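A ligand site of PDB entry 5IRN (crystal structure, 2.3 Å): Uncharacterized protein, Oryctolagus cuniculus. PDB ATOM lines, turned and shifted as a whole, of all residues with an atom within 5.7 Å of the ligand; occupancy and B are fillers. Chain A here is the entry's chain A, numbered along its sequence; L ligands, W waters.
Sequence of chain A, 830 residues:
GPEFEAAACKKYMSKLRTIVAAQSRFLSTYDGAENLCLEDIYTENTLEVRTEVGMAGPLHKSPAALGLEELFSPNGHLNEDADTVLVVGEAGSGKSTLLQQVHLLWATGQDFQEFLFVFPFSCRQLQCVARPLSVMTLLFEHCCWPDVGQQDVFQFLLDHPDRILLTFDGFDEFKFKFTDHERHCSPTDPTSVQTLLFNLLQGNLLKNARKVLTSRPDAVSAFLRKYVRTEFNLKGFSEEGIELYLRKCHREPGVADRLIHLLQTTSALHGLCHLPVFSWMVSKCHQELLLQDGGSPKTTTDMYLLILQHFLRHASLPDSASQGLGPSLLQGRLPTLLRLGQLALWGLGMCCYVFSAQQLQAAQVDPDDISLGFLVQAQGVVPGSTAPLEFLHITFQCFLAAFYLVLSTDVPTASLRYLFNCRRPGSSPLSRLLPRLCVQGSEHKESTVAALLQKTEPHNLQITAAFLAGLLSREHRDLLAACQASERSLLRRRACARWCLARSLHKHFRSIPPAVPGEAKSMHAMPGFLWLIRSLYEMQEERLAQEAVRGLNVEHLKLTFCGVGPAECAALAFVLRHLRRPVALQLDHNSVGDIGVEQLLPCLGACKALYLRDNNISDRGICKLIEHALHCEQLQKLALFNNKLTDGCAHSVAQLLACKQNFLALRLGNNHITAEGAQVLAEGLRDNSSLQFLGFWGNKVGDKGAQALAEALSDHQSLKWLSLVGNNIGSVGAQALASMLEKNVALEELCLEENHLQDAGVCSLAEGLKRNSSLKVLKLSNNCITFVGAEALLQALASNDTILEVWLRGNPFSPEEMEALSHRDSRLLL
Merely in contact with the ligand: Tyr 42 (3.2 Å), Pro 276 (3.4 Å), Tyr 245 (3.5 Å), Trp 280 (3.6 Å), Ile 41 (3.6 Å), Val 277 (3.6 Å), Phe 237 (3.7 Å), Glu 90 (3.7 Å) and Ala 91 (3.8 Å).
Hydrophobic or aromatic side chains that line the ligand: Tyr 42, Phe 237, Tyr 245, Pro 276, Val 277, Trp 280 and His 393.
Of the 25 residues printed, 17 come within 4 Å of the ligand.
The nearest printed residue that does not touch the ligand is Asn 45 (4.03 Å).
The backbone NH (N) of Thr 97 is in hydrogen-bond range of an oxygen (O5) of the ligand (3.0 Å).
O1 of the ligand lies within hydrogen-bond range of NE2 of His 393 (2.8 Å).
An oxygen (O1) of the ligand is in hydrogen-bond range of the backbone NH (N) of Gly 92, 2.8 Å away.
The side-chain amino group (NZ) of Lys 95 lies within salt-bridge range of an oxygen (O2) of the ligand, 2.7 Å away.
The side-chain hydroxyl (OG1) of Thr 97 sits at hydrogen-bond distance from an oxygen (O5) of the ligand, at 2.7 Å.
The backbone NH of Ser 93 is in hydrogen-bond range of an oxygen (O2) of the ligand.
The backbone NH of Thr 43 lies within hydrogen-bond range of a nitrogen (N4) of the ligand (3.1 Å).
The backbone NH of Ser 96 is in hydrogen-bond range of an oxygen (O3) of the ligand, at 2.8 Å.
O of Thr 43 is in hydrogen-bond range of N3 of the ligand (3.1 Å).
The backbone NH (N) of Gly 94 is in hydrogen-bond range of an oxygen (O6) of the ligand (3.1 Å).
The backbone NH (N) of Lys 95 is in hydrogen-bond range of an oxygen (O2) of the ligand (2.8 Å).
The backbone carbonyl oxygen (O) of Glu 90 sits at hydrogen-bond distance from the side-chain amino group (NZ) of Lys 95, 3.2 Å away.
O of Ser 93 is in hydrogen-bond range of ND2 of Asn 45 (2.9 Å).
The backbone carbonyl oxygen (O) of Gly 89 lies within hydrogen-bond range of the side-chain amino group (NZ) of Lys 95 (3.2 Å).
The side-chain carboxylate (OD2) of Asp 169 lies within hydrogen-bond range of the side-chain hydroxyl (OG) of Ser 96.
The backbone carbonyl oxygen of Gly 92 is in hydrogen-bond range of the backbone NH of Val 277 (3.1 Å).
The backbone carbonyl oxygen of Ile 41 lies within hydrogen-bond range of the side-chain hydroxyl of Thr 43 (2.9 Å).
The backbone carbonyl oxygen (O) of Glu 90 is in hydrogen-bond range of the side-chain hydroxyl (OG) of Ser 93.
Water W1 lies within hydrogen-bond range of the side-chain hydroxyl (OH) of Tyr 245 (2.6 Å) and an oxygen (O10) of the ligand (2.7 Å).
Water W3 lies within hydrogen-bond range of the side-chain hydroxyl of Tyr 42 (2.9 Å), the side-chain amide nitrogen of Asn 45 (2.9 Å), the backbone carbonyl oxygen of Gly 94 (2.9 Å) and a nitrogen (N3) of the ligand (3.1 Å).
Water W2 bridges the side-chain amino group of Lys 95 and an oxygen (O1) of the ligand.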
ATOM      1  N   LEU A  27     -29.236 -13.801   7.475  1.00  0.00           N
ATOM      2  CA  LEU A  27     -29.157 -13.116   6.184  1.00  0.00           C
ATOM      3  C   LEU A  27     -29.049 -14.097   5.022  1.00  0.00           C
ATOM      4  O   LEU A  27     -30.021 -14.312   4.306  1.00  0.00           O
ATOM      5  CB  LEU A  27     -28.025 -12.087   6.171  1.00  0.00           C
ATOM      6  CG  LEU A  27     -26.546 -12.481   6.326  1.00  0.00           C
ATOM      7  CD1 LEU A  27     -25.726 -11.197   6.259  1.00  0.00           C
ATOM      8  CD2 LEU A  27     -26.207 -13.283   7.598  1.00  0.00           C
ATOM      9  N   ILE A  41     -21.136 -13.038  11.798  1.00  0.00           N
ATOM     10  CA  ILE A  41     -20.627 -12.741  10.479  1.00  0.00           C
ATOM     11  C   ILE A  41     -20.309 -11.242  10.302  1.00  0.00           C
ATOM     12  O   ILE A  41     -19.366 -10.900   9.616  1.00  0.00           O
ATOM     13  CB  ILE A  41     -21.630 -13.237   9.420  1.00  0.00           C
ATOM     14  CG1 ILE A  41     -21.886 -14.743   9.581  1.00  0.00           C
ATOM     15  CG2 ILE A  41     -21.172 -12.973   8.000  1.00  0.00           C
ATOM     16  CD1 ILE A  41     -20.660 -15.611   9.758  1.00  0.00           C
ATOM     17  N   TYR A  42     -21.043 -10.351  10.945  1.00  0.00           N
ATOM     18  CA  TYR A  42     -20.814  -8.936  10.720  1.00  0.00           C
ATOM     19  C   TYR A  42     -19.375  -8.553  11.066  1.00  0.00           C
ATOM     20  O   TYR A  42     -18.877  -8.924  12.117  1.00  0.00           O
ATOM     21  CB  TYR A  42     -21.777  -8.049  11.484  1.00  0.00           C
ATOM     22  CG  TYR A  42     -21.759  -6.630  11.008  1.00  0.00           C
ATOM     23  CD1 TYR A  42     -22.520  -6.256   9.897  1.00  0.00           C
ATOM     24  CD2 TYR A  42     -20.976  -5.653  11.640  1.00  0.00           C
ATOM     25  CE1 TYR A  42     -22.503  -4.954   9.436  1.00  0.00           C
ATOM     26  CE2 TYR A  42     -20.981  -4.341  11.181  1.00  0.00           C
ATOM     27  CZ  TYR A  42     -21.736  -4.008  10.076  1.00  0.00           C
ATOM     28  OH  TYR A  42     -21.708  -2.737   9.572  1.00  0.00           O
ATOM     29  N   THR A  43     -18.718  -7.814  10.150  1.00  0.00           N
ATOM     30  CA  THR A  43     -17.317  -7.452  10.268  1.00  0.00           C
ATOM     31  C   THR A  43     -17.174  -5.938  10.154  1.00  0.00           C
ATOM     32  O   THR A  43     -17.935  -5.304   9.422  1.00  0.00           O
ATOM     33  CB  THR A  43     -16.534  -8.137   9.134  1.00  0.00           C
ATOM     34  OG1 THR A  43     -16.779  -9.546   9.209  1.00  0.00           O
ATOM     35  CG2 THR A  43     -15.034  -7.830   9.198  1.00  0.00           C
ATOM     36  N   GLU A  44     -16.222  -5.367  10.894  1.00  0.00           N
ATOM     37  CA  GLU A  44     -15.968  -3.918  10.859  1.00  0.00           C
ATOM     38  C   GLU A  44     -16.003  -3.442   9.404  1.00  0.00           C
ATOM     39  O   GLU A  44     -15.434  -4.076   8.508  1.00  0.00           O
ATOM     40  CB  GLU A  44     -14.644  -3.499  11.515  1.00  0.00           C
ATOM     41  CG  GLU A  44     -13.366  -4.210  11.001  1.00  0.00           C
ATOM     42  CD  GLU A  44     -12.101  -3.325  11.025  1.00  0.00           C
ATOM     43  OE1 GLU A  44     -11.243  -3.441  10.088  1.00  0.00           O
ATOM     44  OE2 GLU A  44     -11.988  -2.500  11.995  1.00  0.00           O
ATOM     45  N   ASN A  45     -16.720  -2.349   9.205  1.00  0.00           N
ATOM     46  CA  ASN A  45     -16.833  -1.695   7.933  1.00  0.00           C
ATOM     47  C   ASN A  45     -16.863  -0.231   8.307  1.00  0.00           C
ATOM     48  O   ASN A  45     -17.874   0.268   8.767  1.00  0.00           O
ATOM     49  CB  ASN A  45     -18.110  -2.137   7.228  1.00  0.00           C
ATOM     50  CG  ASN A  45     -18.159  -1.708   5.768  1.00  0.00           C
ATOM     51  OD1 ASN A  45     -17.211  -1.073   5.247  1.00  0.00           O
ATOM     52  ND2 ASN A  45     -19.221  -2.125   5.071  1.00  0.00           N
ATOM     53  N   GLY A  89     -22.664   5.063  -0.053  1.00  0.00           N
ATOM     54  CA  GLY A  89     -21.718   4.031  -0.474  1.00  0.00           C
ATOM     55  C   GLY A  89     -22.129   3.435  -1.803  1.00  0.00           C
ATOM     56  O   GLY A  89     -23.310   3.434  -2.154  1.00  0.00           O
ATOM     57  N   GLU A  90     -21.145   2.936  -2.546  1.00  0.00           N
ATOM     58  CA  GLU A  90     -21.422   2.271  -3.820  1.00  0.00           C
ATOM     59  C   GLU A  90     -22.251   1.035  -3.526  1.00  0.00           C
ATOM     60  O   GLU A  90     -22.269   0.534  -2.376  1.00  0.00           O
ATOM     61  CB  GLU A  90     -20.130   1.815  -4.562  1.00  0.00           C
ATOM     62  CG  GLU A  90     -19.141   2.907  -5.003  1.00  0.00           C
ATOM     63  CD  GLU A  90     -19.758   3.986  -5.899  1.00  0.00           C
ATOM     64  OE1 GLU A  90     -20.571   3.633  -6.783  1.00  0.00           O
ATOM     65  OE2 GLU A  90     -19.436   5.190  -5.701  1.00  0.00           O
ATOM     66  N   ALA A  91     -22.910   0.549  -4.572  1.00  0.00           N
ATOM     67  CA  ALA A  91     -23.578  -0.739  -4.564  1.00  0.00           C
ATOM     68  C   ALA A  91     -22.634  -1.834  -4.131  1.00  0.00           C
ATOM     69  O   ALA A  91     -21.524  -1.948  -4.654  1.00  0.00           O
ATOM     70  CB  ALA A  91     -24.159  -1.067  -5.923  1.00  0.00           C
ATOM     71  N   GLY A  92     -23.050  -2.580  -3.109  1.00  0.00           N
ATOM     72  CA  GLY A  92     -22.342  -3.738  -2.640  1.00  0.00           C
ATOM     73  C   GLY A  92     -21.363  -3.466  -1.549  1.00  0.00           C
ATOM     74  O   GLY A  92     -20.633  -4.388  -1.140  1.00  0.00           O
ATOM     75  N   SER A  93     -21.372  -2.222  -1.039  1.00  0.00           N
ATOM     76  CA  SER A  93     -20.390  -1.784  -0.017  1.00  0.00           C
ATOM     77  C   SER A  93     -20.783  -2.084   1.416  1.00  0.00           C
ATOM     78  O   SER A  93     -19.988  -1.821   2.341  1.00  0.00           O
ATOM     79  CB  SER A  93     -20.142  -0.262  -0.150  1.00  0.00           C
ATOM     80  OG  SER A  93     -21.318   0.518  -0.110  1.00  0.00           O
ATOM     81  N   GLY A  94     -22.013  -2.583   1.605  1.00  0.00           N
ATOM     82  CA  GLY A  94     -22.467  -3.026   2.920  1.00  0.00           C
ATOM     83  C   GLY A  94     -23.517  -2.201   3.653  1.00  0.00           C
ATOM     84  O   GLY A  94     -23.666  -2.354   4.874  1.00  0.00           O
ATOM     85  N   LYS A  95     -24.236  -1.344   2.923  1.00  0.00           N
ATOM     86  CA  LYS A  95     -25.206  -0.389   3.464  1.00  0.00           C
ATOM     87  C   LYS A  95     -26.421  -1.080   4.066  1.00  0.00           C
ATOM     88  O   LYS A  95     -26.742  -0.852   5.213  1.00  0.00           O
ATOM     89  CB  LYS A  95     -25.668   0.599   2.372  1.00  0.00           C
ATOM     90  CG  LYS A  95     -24.539   1.490   1.828  1.00  0.00           C
ATOM     91  CD  LYS A  95     -25.018   2.603   0.907  1.00  0.00           C
ATOM     92  CE  LYS A  95     -25.815   2.145  -0.292  1.00  0.00           C
ATOM     93  NZ  LYS A  95     -25.140   1.076  -1.053  1.00  0.00           N
ATOM     94  N   SER A  96     -27.087  -1.926   3.295  1.00  0.00           N
ATOM     95  CA  SER A  96     -28.128  -2.794   3.839  1.00  0.00           C
ATOM     96  C   SER A  96     -27.714  -3.578   5.070  1.00  0.00           C
ATOM     97  O   SER A  96     -28.496  -3.712   5.995  1.00  0.00           O
ATOM     98  CB  SER A  96     -28.603  -3.777   2.783  1.00  0.00           C
ATOM     99  OG  SER A  96     -29.714  -3.210   2.127  1.00  0.00           O
ATOM    100  N   THR A  97     -26.508  -4.125   5.044  1.00  0.00           N
ATOM    101  CA  THR A  97     -26.054  -5.043   6.102  1.00  0.00           C
ATOM    102  C   THR A  97     -25.723  -4.240   7.346  1.00  0.00           C
ATOM    103  O   THR A  97     -25.989  -4.696   8.449  1.00  0.00           O
ATOM    104  CB  THR A  97     -24.869  -5.877   5.618  1.00  0.00           C
ATOM    105  OG1 THR A  97     -25.190  -6.441   4.347  1.00  0.00           O
ATOM    106  CG2 THR A  97     -24.556  -7.001   6.551  1.00  0.00           C
ATOM    107  N   LEU A  98     -25.191  -3.033   7.164  1.00  0.00           N
ATOM    108  CA  LEU A  98     -25.052  -2.049   8.237  1.00  0.00           C
ATOM    109  C   LEU A  98     -26.381  -1.716   8.949  1.00  0.00           C
ATOM    110  O   LEU A  98     -26.443  -1.719  10.177  1.00  0.00           O
ATOM    111  CB  LEU A  98     -24.425  -0.752   7.734  1.00  0.00           C
ATOM    112  CG  LEU A  98     -24.144   0.340   8.788  1.00  0.00           C
ATOM    113  CD1 LEU A  98     -22.819   1.033   8.545  1.00  0.00           C
ATOM    114  CD2 LEU A  98     -25.236   1.404   8.835  1.00  0.00           C
ATOM    115  N   ASP A 169     -33.809   2.215   3.876  1.00  0.00           N
ATOM    116  CA  ASP A 169     -32.724   1.523   3.195  1.00  0.00           C
ATOM    117  C   ASP A 169     -32.854   1.822   1.701  1.00  0.00           C
ATOM    118  O   ASP A 169     -33.943   1.690   1.160  1.00  0.00           O
ATOM    119  CB  ASP A 169     -32.807   0.028   3.463  1.00  0.00           C
ATOM    120  CG  ASP A 169     -31.569  -0.732   2.951  1.00  0.00           C
ATOM    121  OD1 ASP A 169     -30.530  -0.107   2.653  1.00  0.00           O
ATOM    122  OD2 ASP A 169     -31.651  -1.967   2.879  1.00  0.00           O
ATOM    123  N   LEU A 234     -19.424   4.810   3.363  1.00  0.00           N
ATOM    124  CA  LEU A 234     -19.112   3.427   3.640  1.00  0.00           C
ATOM    125  C   LEU A 234     -18.253   2.923   2.462  1.00  0.00           C
ATOM    126  O   LEU A 234     -18.741   2.788   1.339  1.00  0.00           O
ATOM    127  CB  LEU A 234     -20.438   2.669   3.792  1.00  0.00           C
ATOM    128  CG  LEU A 234     -20.346   1.291   4.418  1.00  0.00           C
ATOM    129  CD1 LEU A 234     -19.836   1.390   5.850  1.00  0.00           C
ATOM    130  CD2 LEU A 234     -21.698   0.629   4.337  1.00  0.00           C
ATOM    131  N   PHE A 237     -14.475  -3.260   3.254  1.00  0.00           N
ATOM    132  CA  PHE A 237     -13.551  -3.899   4.176  1.00  0.00           C
ATOM    133  C   PHE A 237     -12.136  -3.412   3.883  1.00  0.00           C
ATOM    134  O   PHE A 237     -11.742  -3.304   2.722  1.00  0.00           O
ATOM    135  CB  PHE A 237     -13.535  -5.415   4.057  1.00  0.00           C
ATOM    136  CG  PHE A 237     -14.833  -6.100   4.416  1.00  0.00           C
ATOM    137  CD1 PHE A 237     -15.675  -5.615   5.401  1.00  0.00           C
ATOM    138  CD2 PHE A 237     -15.144  -7.301   3.791  1.00  0.00           C
ATOM    139  CE1 PHE A 237     -16.839  -6.271   5.719  1.00  0.00           C
ATOM    140  CE2 PHE A 237     -16.299  -7.969   4.111  1.00  0.00           C
ATOM    141  CZ  PHE A 237     -17.150  -7.466   5.073  1.00  0.00           C
ATOM    142  N   TYR A 245     -13.373 -11.345   8.128  1.00  0.00           N
ATOM    143  CA  TYR A 245     -14.591 -11.840   7.506  1.00  0.00           C
ATOM    144  C   TYR A 245     -14.474 -13.309   7.123  1.00  0.00           C
ATOM    145  O   TYR A 245     -15.423 -14.096   7.287  1.00  0.00           O
ATOM    146  CB  TYR A 245     -14.937 -11.023   6.263  1.00  0.00           C
ATOM    147  CG  TYR A 245     -16.132 -11.568   5.513  1.00  0.00           C
ATOM    148  CD1 TYR A 245     -17.430 -11.289   5.945  1.00  0.00           C
ATOM    149  CD2 TYR A 245     -15.974 -12.387   4.409  1.00  0.00           C
ATOM    150  CE1 TYR A 245     -18.529 -11.779   5.256  1.00  0.00           C
ATOM    151  CE2 TYR A 245     -17.067 -12.917   3.726  1.00  0.00           C
ATOM    152  CZ  TYR A 245     -18.347 -12.597   4.158  1.00  0.00           C
ATOM    153  OH  TYR A 245     -19.440 -13.077   3.514  1.00  0.00           O
ATOM    154  N   PRO A 276     -17.453  -5.598   0.227  1.00  0.00           N
ATOM    155  CA  PRO A 276     -18.011  -6.783   0.913  1.00  0.00           C
ATOM    156  C   PRO A 276     -18.771  -7.763   0.018  1.00  0.00           C
ATOM    157  O   PRO A 276     -18.674  -8.971   0.220  1.00  0.00           O
ATOM    158  CB  PRO A 276     -18.899  -6.171   1.975  1.00  0.00           C
ATOM    159  CG  PRO A 276     -18.143  -4.948   2.361  1.00  0.00           C
ATOM    160  CD  PRO A 276     -17.544  -4.404   1.086  1.00  0.00           C
ATOM    161  N   VAL A 277     -19.446  -7.267  -1.001  1.00  0.00           N
ATOM    162  CA  VAL A 277     -20.145  -8.168  -1.870  1.00  0.00           C
ATOM    163  C   VAL A 277     -19.186  -9.189  -2.512  1.00  0.00           C
ATOM    164  O   VAL A 277     -19.610 -10.326  -2.686  1.00  0.00           O
ATOM    165  CB  VAL A 277     -21.004  -7.444  -2.945  1.00  0.00           C
ATOM    166  CG1 VAL A 277     -20.140  -6.766  -3.999  1.00  0.00           C
ATOM    167  CG2 VAL A 277     -21.987  -8.433  -3.580  1.00  0.00           C
ATOM    168  N   TRP A 280     -18.053 -11.868  -0.018  1.00  0.00           N
ATOM    169  CA  TRP A 280     -19.145 -12.833   0.043  1.00  0.00           C
ATOM    170  C   TRP A 280     -19.043 -13.868  -1.080  1.00  0.00           C
ATOM    171  O   TRP A 280     -19.147 -15.074  -0.828  1.00  0.00           O
ATOM    172  CB  TRP A 280     -20.528 -12.154  -0.014  1.00  0.00           C
ATOM    173  CG  TRP A 280     -21.675 -13.133  -0.090  1.00  0.00           C
ATOM    174  CD1 TRP A 280     -22.186 -13.880   0.939  1.00  0.00           C
ATOM    175  CD2 TRP A 280     -22.409 -13.502  -1.254  1.00  0.00           C
ATOM    176  NE1 TRP A 280     -23.185 -14.687   0.494  1.00  0.00           N
ATOM    177  CE2 TRP A 280     -23.365 -14.463  -0.842  1.00  0.00           C
ATOM    178  CE3 TRP A 280     -22.415 -13.076  -2.574  1.00  0.00           C
ATOM    179  CZ2 TRP A 280     -24.270 -15.041  -1.724  1.00  0.00           C
ATOM    180  CZ3 TRP A 280     -23.333 -13.627  -3.443  1.00  0.00           C
ATOM    181  CH2 TRP A 280     -24.248 -14.609  -3.022  1.00  0.00           C
ATOM    182  N   HIS A 393     -29.225  -9.208  -5.322  1.00  0.00           N
ATOM    183  CA  HIS A 393     -28.661  -7.881  -5.075  1.00  0.00           C
ATOM    184  C   HIS A 393     -28.851  -7.045  -6.362  1.00  0.00           C
ATOM    185  O   HIS A 393     -28.960  -7.586  -7.466  1.00  0.00           O
ATOM    186  CB  HIS A 393     -27.168  -8.015  -4.734  1.00  0.00           C
ATOM    187  CG  HIS A 393     -26.551  -6.749  -4.210  1.00  0.00           C
ATOM    188  ND1 HIS A 393     -25.681  -5.976  -4.952  1.00  0.00           N
ATOM    189  CD2 HIS A 393     -26.665  -6.129  -3.014  1.00  0.00           C
ATOM    190  CE1 HIS A 393     -25.291  -4.936  -4.232  1.00  0.00           C
ATOM    191  NE2 HIS A 393     -25.881  -5.006  -3.049  1.00  0.00           N
ATOM    192  N   ILE A 394     -28.893  -5.728  -6.232  1.00  0.00           N
ATOM    193  CA  ILE A 394     -29.105  -4.877  -7.392  1.00  0.00           C
ATOM    194  C   ILE A 394     -28.041  -5.111  -8.485  1.00  0.00           C
ATOM    195  O   ILE A 394     -28.363  -5.024  -9.665  1.00  0.00           O
ATOM    196  CB  ILE A 394     -29.243  -3.393  -6.976  1.00  0.00           C
ATOM    197  CG1 ILE A 394     -29.768  -2.544  -8.142  1.00  0.00           C
ATOM    198  CG2 ILE A 394     -27.917  -2.835  -6.449  1.00  0.00           C
ATOM    199  CD1 ILE A 394     -31.164  -2.929  -8.638  1.00  0.00           C
HETATM  200  P1  LIG L   1     -25.275  -2.416  -0.252  1.00  0.00           P
HETATM  201  O1  LIG L   1     -25.456  -2.607  -1.744  1.00  0.00           O
HETATM  202  O2  LIG L   1     -24.351  -1.283   0.080  1.00  0.00           O
HETATM  203  O3  LIG L   1     -26.506  -2.419   0.622  1.00  0.00           O
HETATM  204  P2  LIG L   1     -25.078  -5.026   0.993  1.00  0.00           P
HETATM  205  O4  LIG L   1     -26.232  -5.597   0.221  1.00  0.00           O
HETATM  206  O5  LIG L   1     -25.177  -4.566   2.415  1.00  0.00           O
HETATM  207  O6  LIG L   1     -24.465  -3.740   0.195  1.00  0.00           O
HETATM  208  O7  LIG L   1     -23.811  -5.977   0.891  1.00  0.00           O
HETATM  209  C1  LIG L   1     -23.620  -7.035  -0.017  1.00  0.00           C
HETATM  210  C2  LIG L   1     -23.280  -8.311   0.746  1.00  0.00           C
HETATM  211  O8  LIG L   1     -21.972  -8.283   1.323  1.00  0.00           O
HETATM  212  C3  LIG L   1     -24.226  -8.628   1.891  1.00  0.00           C
HETATM  213  O9  LIG L   1     -25.345  -9.374   1.458  1.00  0.00           O
HETATM  214  C4  LIG L   1     -23.394  -9.481   2.821  1.00  0.00           C
HETATM  215  O10 LIG L   1     -23.361 -10.829   2.339  1.00  0.00           O
HETATM  216  C5  LIG L   1     -22.036  -8.881   2.638  1.00  0.00           C
HETATM  217  N1  LIG L   1     -21.739  -7.855   3.634  1.00  0.00           N
HETATM  218  C6  LIG L   1     -21.906  -6.504   3.504  1.00  0.00           C
HETATM  219  N2  LIG L   1     -21.485  -5.810   4.602  1.00  0.00           N
HETATM  220  C7  LIG L   1     -21.018  -6.763   5.429  1.00  0.00           C
HETATM  221  C8  LIG L   1     -20.414  -6.750   6.731  1.00  0.00           C
HETATM  222  N3  LIG L   1     -20.227  -5.567   7.333  1.00  0.00           N
HETATM  223  N4  LIG L   1     -20.034  -7.910   7.292  1.00  0.00           N
HETATM  224  C9  LIG L   1     -20.216  -9.074   6.663  1.00  0.00           C
HETATM  225  N5  LIG L   1     -20.796  -9.183   5.462  1.00  0.00           N
HETATM  226  C10 LIG L   1     -21.186  -8.077   4.808  1.00  0.00           C
HETATM  227  O   HOH W   1     -21.605 -11.770   4.188  1.00  0.00           O
HETATM  228  O   HOH W   2     -26.572   0.057  -3.021  1.00  0.00           O
HETATM  229  O   HOH W   3     -21.475  -2.821   6.713  1.00  0.00           O
